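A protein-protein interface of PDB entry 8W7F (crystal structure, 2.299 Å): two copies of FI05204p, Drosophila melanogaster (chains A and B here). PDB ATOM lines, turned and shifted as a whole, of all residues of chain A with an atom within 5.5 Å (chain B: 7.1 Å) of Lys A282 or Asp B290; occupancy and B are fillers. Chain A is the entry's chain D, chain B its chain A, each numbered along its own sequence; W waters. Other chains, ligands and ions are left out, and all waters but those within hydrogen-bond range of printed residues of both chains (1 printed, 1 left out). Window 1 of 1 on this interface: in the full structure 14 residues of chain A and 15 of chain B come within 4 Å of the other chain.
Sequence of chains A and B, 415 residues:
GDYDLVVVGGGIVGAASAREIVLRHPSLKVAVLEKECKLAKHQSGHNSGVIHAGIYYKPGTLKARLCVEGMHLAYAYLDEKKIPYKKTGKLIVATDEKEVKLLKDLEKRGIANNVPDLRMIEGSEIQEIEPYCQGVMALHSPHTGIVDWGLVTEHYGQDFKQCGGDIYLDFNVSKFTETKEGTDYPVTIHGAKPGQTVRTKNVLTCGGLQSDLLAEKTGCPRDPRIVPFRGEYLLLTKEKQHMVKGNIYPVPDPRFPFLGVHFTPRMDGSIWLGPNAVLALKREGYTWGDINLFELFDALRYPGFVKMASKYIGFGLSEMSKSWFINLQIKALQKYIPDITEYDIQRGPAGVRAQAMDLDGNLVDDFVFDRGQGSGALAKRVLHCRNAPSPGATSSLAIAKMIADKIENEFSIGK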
ATOM      1  N   PRO A 228     -16.232  15.565  -6.243  1.00  0.00           N
ATOM      2  CA  PRO A 228     -15.246  16.544  -6.719  1.00  0.00           C
ATOM      3  C   PRO A 228     -13.872  16.294  -6.111  1.00  0.00           C
ATOM      4  O   PRO A 228     -13.730  16.166  -4.892  1.00  0.00           O
ATOM      5  CB  PRO A 228     -15.829  17.885  -6.257  1.00  0.00           C
ATOM      6  CG  PRO A 228     -16.655  17.539  -5.061  1.00  0.00           C
ATOM      7  CD  PRO A 228     -17.206  16.158  -5.308  1.00  0.00           C
ATOM      8  N   ALA A 280     -12.520  17.645  -2.511  1.00  0.00           N
ATOM      9  CA  ALA A 280     -13.151  18.941  -2.338  1.00  0.00           C
ATOM     10  C   ALA A 280     -14.498  18.767  -1.655  1.00  0.00           C
ATOM     11  O   ALA A 280     -15.184  17.757  -1.837  1.00  0.00           O
ATOM     12  CB  ALA A 280     -13.328  19.647  -3.683  1.00  0.00           C
ATOM     13  N   LEU A 281     -14.868  19.756  -0.849  1.00  0.00           N
ATOM     14  CA  LEU A 281     -16.157  19.746  -0.160  1.00  0.00           C
ATOM     15  C   LEU A 281     -17.151  20.675  -0.840  1.00  0.00           C
ATOM     16  O   LEU A 281     -17.995  21.297  -0.189  1.00  0.00           O
ATOM     17  CB  LEU A 281     -15.974  20.105   1.310  1.00  0.00           C
ATOM     18  CG  LEU A 281     -15.202  19.026   2.079  1.00  0.00           C
ATOM     19  CD1 LEU A 281     -15.004  19.421   3.533  1.00  0.00           C
ATOM     20  CD2 LEU A 281     -15.906  17.675   1.973  1.00  0.00           C
ATOM     21  N   LYS A 282     -17.061  20.760  -2.165  1.00  0.00           N
ATOM     22  CA  LYS A 282     -17.907  21.602  -2.997  1.00  0.00           C
ATOM     23  C   LYS A 282     -17.672  21.208  -4.448  1.00  0.00           C
ATOM     24  O   LYS A 282     -16.524  21.012  -4.854  1.00  0.00           O
ATOM     25  CB  LYS A 282     -17.593  23.087  -2.784  1.00  0.00           C
ATOM     26  CG  LYS A 282     -18.368  24.028  -3.691  1.00  0.00           C
ATOM     27  CD  LYS A 282     -17.930  25.466  -3.468  1.00  0.00           C
ATOM     28  CE  LYS A 282     -18.769  26.439  -4.271  1.00  0.00           C
ATOM     29  NZ  LYS A 282     -18.440  27.845  -3.904  1.00  0.00           N
ATOM     30  N   ARG A 283     -18.758  21.087  -5.214  1.00  0.00           N
ATOM     31  CA  ARG A 283     -18.640  20.673  -6.610  1.00  0.00           C
ATOM     32  C   ARG A 283     -17.679  21.579  -7.370  1.00  0.00           C
ATOM     33  O   ARG A 283     -16.789  21.106  -8.084  1.00  0.00           O
ATOM     34  CB  ARG A 283     -20.016  20.665  -7.277  1.00  0.00           C
ATOM     35  CG  ARG A 283     -20.971  19.624  -6.723  1.00  0.00           C
ATOM     36  CD  ARG A 283     -20.409  18.223  -6.868  1.00  0.00           C
ATOM     37  NE  ARG A 283     -21.343  17.208  -6.385  1.00  0.00           N
ATOM     38  CZ  ARG A 283     -22.210  16.565  -7.159  1.00  0.00           C
ATOM     39  NH1 ARG A 283     -22.267  16.830  -8.457  1.00  0.00           N
ATOM     40  NH2 ARG A 283     -23.021  15.657  -6.634  1.00  0.00           N
ATOM     41  N   GLU A 284     -17.833  22.891  -7.211  1.00  0.00           N
ATOM     42  CA  GLU A 284     -16.907  23.869  -7.776  1.00  0.00           C
ATOM     43  C   GLU A 284     -15.976  24.435  -6.711  1.00  0.00           C
ATOM     44  O   GLU A 284     -15.708  25.640  -6.672  1.00  0.00           O
ATOM     45  CB  GLU A 284     -17.677  24.983  -8.479  1.00  0.00           C
ATOM     46  CG  GLU A 284     -18.642  24.457  -9.535  1.00  0.00           C
ATOM     47  CD  GLU A 284     -19.295  25.556 -10.352  1.00  0.00           C
ATOM     48  OE1 GLU A 284     -19.066  26.745 -10.046  1.00  0.00           O
ATOM     49  OE2 GLU A 284     -20.036  25.226 -11.303  1.00  0.00           O
ATOM     50  N   GLY A 285     -15.468  23.574  -5.832  1.00  0.00           N
ATOM     51  CA  GLY A 285     -14.557  24.002  -4.790  1.00  0.00           C
ATOM     52  C   GLY A 285     -13.149  24.225  -5.297  1.00  0.00           C
ATOM     53  O   GLY A 285     -12.265  23.390  -5.086  1.00  0.00           O
ATOM     54  N   ASP A 290     -13.583  26.935   0.646  1.00  0.00           N
ATOM     55  CA  ASP A 290     -14.811  27.255  -0.079  1.00  0.00           C
ATOM     56  C   ASP A 290     -15.627  25.974  -0.155  1.00  0.00           C
ATOM     57  O   ASP A 290     -15.483  25.171  -1.078  1.00  0.00           O
ATOM     58  CB  ASP A 290     -14.498  27.813  -1.461  1.00  0.00           C
ATOM     59  CG  ASP A 290     -15.591  28.719  -1.978  1.00  0.00           C
ATOM     60  OD1 ASP A 290     -15.994  29.639  -1.235  1.00  0.00           O
ATOM     61  OD2 ASP A 290     -16.049  28.516  -3.124  1.00  0.00           O
ATOM     62  N   ILE A 291     -16.493  25.777   0.835  1.00  0.00           N
ATOM     63  CA  ILE A 291     -17.230  24.533   0.978  1.00  0.00           C
ATOM     64  C   ILE A 291     -18.721  24.806   0.814  1.00  0.00           C
ATOM     65  O   ILE A 291     -19.186  25.947   0.859  1.00  0.00           O
ATOM     66  CB  ILE A 291     -16.949  23.841   2.326  1.00  0.00           C
ATOM     67  CG1 ILE A 291     -17.736  24.516   3.449  1.00  0.00           C
ATOM     68  CG2 ILE A 291     -15.462  23.860   2.632  1.00  0.00           C
ATOM     69  CD1 ILE A 291     -17.489  23.916   4.819  1.00  0.00           C
ATOM     70  N   ASN A 292     -19.462  23.724   0.601  1.00  0.00           N
ATOM     71  CA  ASN A 292     -20.917  23.714   0.596  1.00  0.00           C
ATOM     72  C   ASN A 292     -21.367  22.590   1.516  1.00  0.00           C
ATOM     73  O   ASN A 292     -20.940  21.444   1.353  1.00  0.00           O
ATOM     74  CB  ASN A 292     -21.469  23.508  -0.816  1.00  0.00           C
ATOM     75  CG  ASN A 292     -22.982  23.503  -0.854  1.00  0.00           C
ATOM     76  OD1 ASN A 292     -23.614  22.481  -0.597  1.00  0.00           O
ATOM     77  ND2 ASN A 292     -23.573  24.646  -1.190  1.00  0.00           N
ATOM     78  N   LEU A 293     -22.210  22.916   2.497  1.00  0.00           N
ATOM     79  CA  LEU A 293     -22.561  21.921   3.509  1.00  0.00           C
ATOM     80  C   LEU A 293     -23.499  20.860   2.970  1.00  0.00           C
ATOM     81  O   LEU A 293     -23.475  19.718   3.449  1.00  0.00           O
ATOM     82  CB  LEU A 293     -23.170  22.586   4.746  1.00  0.00           C
ATOM     83  CG  LEU A 293     -22.284  23.579   5.466  1.00  0.00           C
ATOM     84  CD1 LEU A 293     -23.149  24.425   6.382  1.00  0.00           C
ATOM     85  CD2 LEU A 293     -21.161  22.868   6.224  1.00  0.00           C
ATOM     86  N   GLU A 295     -23.231  19.693  -0.018  1.00  0.00           N
ATOM     87  CA  GLU A 295     -22.276  18.791  -0.646  1.00  0.00           C
ATOM     88  C   GLU A 295     -21.573  17.923   0.388  1.00  0.00           C
ATOM     89  O   GLU A 295     -21.267  16.758   0.113  1.00  0.00           O
ATOM     90  CB  GLU A 295     -21.254  19.588  -1.460  1.00  0.00           C
ATOM     91  CG  GLU A 295     -20.091  18.761  -1.988  1.00  0.00           C
ATOM     92  CD  GLU A 295     -20.523  17.683  -2.969  1.00  0.00           C
ATOM     93  OE1 GLU A 295     -21.581  17.846  -3.616  1.00  0.00           O
ATOM     94  OE2 GLU A 295     -19.799  16.675  -3.103  1.00  0.00           O
ATOM     95  N   VAL A 352     -11.005  21.119 -10.676  1.00  0.00           N
ATOM     96  CA  VAL A 352     -11.815  20.173  -9.917  1.00  0.00           C
ATOM     97  C   VAL A 352     -12.258  19.059 -10.854  1.00  0.00           C
ATOM     98  O   VAL A 352     -13.000  19.309 -11.811  1.00  0.00           O
ATOM     99  CB  VAL A 352     -13.037  20.845  -9.266  1.00  0.00           C
ATOM    100  CG1 VAL A 352     -13.760  19.856  -8.385  1.00  0.00           C
ATOM    101  CG2 VAL A 352     -12.616  22.065  -8.454  1.00  0.00           C
ATOM    102  N   ARG B 230     -27.432  37.885   2.231  1.00  0.00           N
ATOM    103  CA  ARG B 230     -28.091  37.109   1.190  1.00  0.00           C
ATOM    104  C   ARG B 230     -29.549  37.527   1.049  1.00  0.00           C
ATOM    105  O   ARG B 230     -30.272  37.645   2.044  1.00  0.00           O
ATOM    106  CB  ARG B 230     -28.002  35.619   1.512  1.00  0.00           C
ATOM    107  CG  ARG B 230     -27.986  34.716   0.303  1.00  0.00           C
ATOM    108  CD  ARG B 230     -27.497  33.331   0.684  1.00  0.00           C
ATOM    109  NE  ARG B 230     -28.603  32.417   0.923  1.00  0.00           N
ATOM    110  CZ  ARG B 230     -29.161  31.667  -0.020  1.00  0.00           C
ATOM    111  NH1 ARG B 230     -30.169  30.860   0.282  1.00  0.00           N
ATOM    112  NH2 ARG B 230     -28.707  31.722  -1.266  1.00  0.00           N
ATOM    113  N   ALA B 280     -24.848  36.234   5.023  1.00  0.00           N
ATOM    114  CA  ALA B 280     -24.218  35.275   4.130  1.00  0.00           C
ATOM    115  C   ALA B 280     -22.906  34.785   4.724  1.00  0.00           C
ATOM    116  O   ALA B 280     -22.140  35.560   5.304  1.00  0.00           O
ATOM    117  CB  ALA B 280     -23.975  35.898   2.755  1.00  0.00           C
ATOM    118  N   LEU B 281     -22.658  33.489   4.581  1.00  0.00           N
ATOM    119  CA  LEU B 281     -21.421  32.873   5.034  1.00  0.00           C
ATOM    120  C   LEU B 281     -20.345  32.889   3.957  1.00  0.00           C
ATOM    121  O   LEU B 281     -19.342  32.175   4.079  1.00  0.00           O
ATOM    122  CB  LEU B 281     -21.703  31.444   5.502  1.00  0.00           C
ATOM    123  CG  LEU B 281     -23.003  31.359   6.310  1.00  0.00           C
ATOM    124  CD1 LEU B 281     -23.498  29.931   6.461  1.00  0.00           C
ATOM    125  CD2 LEU B 281     -22.829  32.012   7.675  1.00  0.00           C
ATOM    126  N   LYS B 282     -20.533  33.691   2.914  1.00  0.00           N
ATOM    127  CA  LYS B 282     -19.581  33.820   1.822  1.00  0.00           C
ATOM    128  C   LYS B 282     -19.882  35.124   1.099  1.00  0.00           C
ATOM    129  O   LYS B 282     -21.050  35.495   0.964  1.00  0.00           O
ATOM    130  CB  LYS B 282     -19.671  32.627   0.863  1.00  0.00           C
ATOM    131  CG  LYS B 282     -19.074  32.884  -0.506  1.00  0.00           C
ATOM    132  CD  LYS B 282     -18.942  31.614  -1.325  1.00  0.00           C
ATOM    133  CE  LYS B 282     -18.017  31.859  -2.503  1.00  0.00           C
ATOM    134  NZ  LYS B 282     -17.774  30.645  -3.304  1.00  0.00           N
ATOM    135  N   GLU B 284     -19.598  36.051  -2.174  1.00  0.00           N
ATOM    136  CA  GLU B 284     -20.476  35.713  -3.291  1.00  0.00           C
ATOM    137  C   GLU B 284     -21.273  34.449  -2.992  1.00  0.00           C
ATOM    138  O   GLU B 284     -21.305  33.499  -3.772  1.00  0.00           O
ATOM    139  CB  GLU B 284     -19.659  35.570  -4.570  1.00  0.00           C
ATOM    140  CG  GLU B 284     -18.950  36.856  -4.973  1.00  0.00           C
ATOM    141  CD  GLU B 284     -18.042  36.678  -6.173  1.00  0.00           C
ATOM    142  OE1 GLU B 284     -18.019  35.569  -6.744  1.00  0.00           O
ATOM    143  OE2 GLU B 284     -17.355  37.652  -6.550  1.00  0.00           O
ATOM    144  N   GLY B 285     -21.925  34.439  -1.833  1.00  0.00           N
ATOM    145  CA  GLY B 285     -22.707  33.293  -1.413  1.00  0.00           C
ATOM    146  C   GLY B 285     -24.103  33.269  -1.996  1.00  0.00           C
ATOM    147  O   GLY B 285     -25.087  33.413  -1.270  1.00  0.00           O
ATOM    148  N   TYR B 286     -24.205  33.090  -3.315  1.00  0.00           N
ATOM    149  CA  TYR B 286     -25.517  32.989  -3.943  1.00  0.00           C
ATOM    150  C   TYR B 286     -26.153  31.634  -3.661  1.00  0.00           C
ATOM    151  O   TYR B 286     -27.338  31.550  -3.314  1.00  0.00           O
ATOM    152  CB  TYR B 286     -25.398  33.227  -5.448  1.00  0.00           C
ATOM    153  CG  TYR B 286     -24.839  34.582  -5.798  1.00  0.00           C
ATOM    154  CD1 TYR B 286     -25.676  35.673  -5.975  1.00  0.00           C
ATOM    155  CD2 TYR B 286     -23.472  34.773  -5.944  1.00  0.00           C
ATOM    156  CE1 TYR B 286     -25.170  36.917  -6.293  1.00  0.00           C
ATOM    157  CE2 TYR B 286     -22.957  36.012  -6.260  1.00  0.00           C
ATOM    158  CZ  TYR B 286     -23.810  37.079  -6.434  1.00  0.00           C
ATOM    159  OH  TYR B 286     -23.300  38.315  -6.746  1.00  0.00           O
ATOM    160  N   THR B 287     -25.380  30.561  -3.813  1.00  0.00           N
ATOM    161  CA  THR B 287     -25.865  29.229  -3.481  1.00  0.00           C
ATOM    162  C   THR B 287     -26.126  29.129  -1.984  1.00  0.00           C
ATOM    163  O   THR B 287     -25.395  29.704  -1.172  1.00  0.00           O
ATOM    164  CB  THR B 287     -24.849  28.172  -3.919  1.00  0.00           C
ATOM    165  OG1 THR B 287     -24.358  28.495  -5.228  1.00  0.00           O
ATOM    166  CG2 THR B 287     -25.487  26.787  -3.952  1.00  0.00           C
ATOM    167  N   TRP B 288     -27.176  28.393  -1.624  1.00  0.00           N
ATOM    168  CA  TRP B 288     -27.668  28.358  -0.251  1.00  0.00           C
ATOM    169  C   TRP B 288     -26.601  27.913   0.743  1.00  0.00           C
ATOM    170  O   TRP B 288     -26.178  28.702   1.593  1.00  0.00           O
ATOM    171  CB  TRP B 288     -28.891  27.443  -0.154  1.00  0.00           C
ATOM    172  CG  TRP B 288     -29.627  27.556   1.147  1.00  0.00           C
ATOM    173  CD1 TRP B 288     -29.370  28.433   2.164  1.00  0.00           C
ATOM    174  CD2 TRP B 288     -30.742  26.765   1.572  1.00  0.00           C
ATOM    175  NE1 TRP B 288     -30.256  28.234   3.194  1.00  0.00           N
ATOM    176  CE2 TRP B 288     -31.109  27.217   2.857  1.00  0.00           C
ATOM    177  CE3 TRP B 288     -31.465  25.719   0.992  1.00  0.00           C
ATOM    178  CZ2 TRP B 288     -32.167  26.657   3.569  1.00  0.00           C
ATOM    179  CZ3 TRP B 288     -32.515  25.166   1.699  1.00  0.00           C
ATOM    180  CH2 TRP B 288     -32.854  25.634   2.977  1.00  0.00           C
ATOM    181  N   GLY B 289     -26.165  26.661   0.654  1.00  0.00           N
ATOM    182  CA  GLY B 289     -25.244  26.133   1.639  1.00  0.00           C
ATOM    183  C   GLY B 289     -23.789  26.496   1.457  1.00  0.00           C
ATOM    184  O   GLY B 289     -22.933  25.924   2.141  1.00  0.00           O
ATOM    185  N   ASP B 290     -23.471  27.431   0.564  1.00  0.00           N
ATOM    186  CA  ASP B 290     -22.079  27.764   0.293  1.00  0.00           C
ATOM    187  C   ASP B 290     -21.471  28.519   1.469  1.00  0.00           C
ATOM    188  O   ASP B 290     -22.044  29.497   1.958  1.00  0.00           O
ATOM    189  CB  ASP B 290     -21.963  28.594  -0.983  1.00  0.00           C
ATOM    190  CG  ASP B 290     -21.698  27.745  -2.210  1.00  0.00           C
ATOM    191  OD1 ASP B 290     -21.876  26.509  -2.136  1.00  0.00           O
ATOM    192  OD2 ASP B 290     -21.303  28.315  -3.250  1.00  0.00           O
ATOM    193  N   ILE B 291     -20.303  28.064   1.913  1.00  0.00           N
ATOM    194  CA  ILE B 291     -19.591  28.659   3.035  1.00  0.00           C
ATOM    195  C   ILE B 291     -18.138  28.859   2.642  1.00  0.00           C
ATOM    196  O   ILE B 291     -17.508  27.950   2.092  1.00  0.00           O
ATOM    197  CB  ILE B 291     -19.670  27.791   4.306  1.00  0.00           C
ATOM    198  CG1 ILE B 291     -21.084  27.781   4.876  1.00  0.00           C
ATOM    199  CG2 ILE B 291     -18.704  28.295   5.359  1.00  0.00           C
ATOM    200  CD1 ILE B 291     -21.134  27.321   6.321  1.00  0.00           C
ATOM    201  N   ASN B 292     -17.604  30.038   2.936  1.00  0.00           N
ATOM    202  CA  ASN B 292     -16.172  30.288   2.863  1.00  0.00           C
ATOM    203  C   ASN B 292     -15.663  30.547   4.273  1.00  0.00           C
ATOM    204  O   ASN B 292     -16.100  31.500   4.927  1.00  0.00           O
ATOM    205  CB  ASN B 292     -15.857  31.466   1.946  1.00  0.00           C
ATOM    206  CG  ASN B 292     -14.425  31.449   1.466  1.00  0.00           C
ATOM    207  OD1 ASN B 292     -13.539  32.007   2.108  1.00  0.00           O
ATOM    208  ND2 ASN B 292     -14.185  30.789   0.339  1.00  0.00           N
HETATM  209  O   HOH W   1     -16.645  31.020  -5.461  1.00  0.00           O
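The side-chain amino group (NZ) of Lys B282 is in salt-bridge range of the side-chain carboxylate (OD2) of Asp A290 (2.7 Å). The backbone carbonyl oxygen of Gly B289 lies within hydrogen-bond range of the backbone NH of Leu A293. The side-chain amino group (NZ) of Lys A282 lies within salt-bridge range of the side-chain carboxylate (OD2) of Asp B290 (3.0 Å). The side-chain amide nitrogen of Asn A292 is in hydrogen-bond range of the side-chain carboxylate of Asp B290. The backbone carbonyl oxygen of Ile A291 is in hydrogen-bond range of the backbone NH of Ile B291 (2.6 Å). OD1 of Asp A290 sits at hydrogen-bond distance from ND2 of Asn B292, at 2.7 Å. The side-chain amino group (NZ) of Lys B282 sits close to the side-chain amino group (NZ) of Lys A282 (2.9 Å).
N of Asn B292 lies within hydrogen-bond range of O of Leu B281, 3.0 Å away. The backbone carbonyl oxygen (O) of Leu A281 is in hydrogen-bond range of the backbone NH (N) of Asn A292. OD2 of Asp A290 lies within salt-bridge range of NZ of Lys A282, at 2.6 Å. The backbone NH (N) of Glu A295 lies within hydrogen-bond range of the side-chain amide oxygen (OD1) of Asn A292.
Of the 13 printed residues of chain A, 5 touch a printed residue of chain B. Printed residues of chain A that touch a printed residue of chain B: Lys A282, Asp A290, Ile A291, Asn A292 and Leu A293. Along chain A the printed residues that touch a printed residue of chain B span positions 282 to 293. Among the printed residues, Asp or Glu carboxylates within 4 Å of a Lys or Arg side-chain nitrogen of the other chain: Lys A282 with Asp B290 (3.0 Å) and Asp A290 with Lys B282 (2.7 Å).
Lys A282 touches its own counterpart, Lys B282. Lys A282 touches Asp B290, and with the chains exchanged Asp A290 touches Lys B282. Asp A290 touches Ile B291, and with the chains exchanged Ile A291 touches Asp B290. Asp A290 touches Asn B292, and with the chains exchanged Asn A292 touches Asp B290. Positions printed for both chains: 280, 281, 282, 284, 285, 290, 291 and 292.
Water W1 lies within hydrogen-bond range of the side-chain amino group of Lys B282 (2.5 Å) and the side-chain carboxylate of Asp A290 (3.5 Å).
Lys A282 touches just these residues of chain B: Lys B282 and Asp B290. Asp B290 touches three residues of chain A. Printed residues of chain A within 4 Å of Asn B292: Asp A290 (2.7 Å). Of the printed residues of chain A, Gly B289 touches Ile A291, Asn A292 and Leu A293. Of the printed residues of chain A, Thr B287 touches Asn A292. Printed residues of chain B within 4 Å of Asp A290: Lys B282 (2.7 Å), Ile B291 (3.5 Å) and Asn B292 (2.7 Å). The nearest residue of chain B that does not touch Lys A282 is Thr B287 (6.0 Å).
Asp A290 touches Ile B291. Ile A291 touches Gly B289 (O to O, 3.96 Å). Asp B290 touches Ile A291. CG2 of Thr B287 touches ND2 of Asn A292, 3.98 Å away. ND2 of Asn A292 touches C of Gly B289, 3.2 Å away. Ile B291 touches Leu A293.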
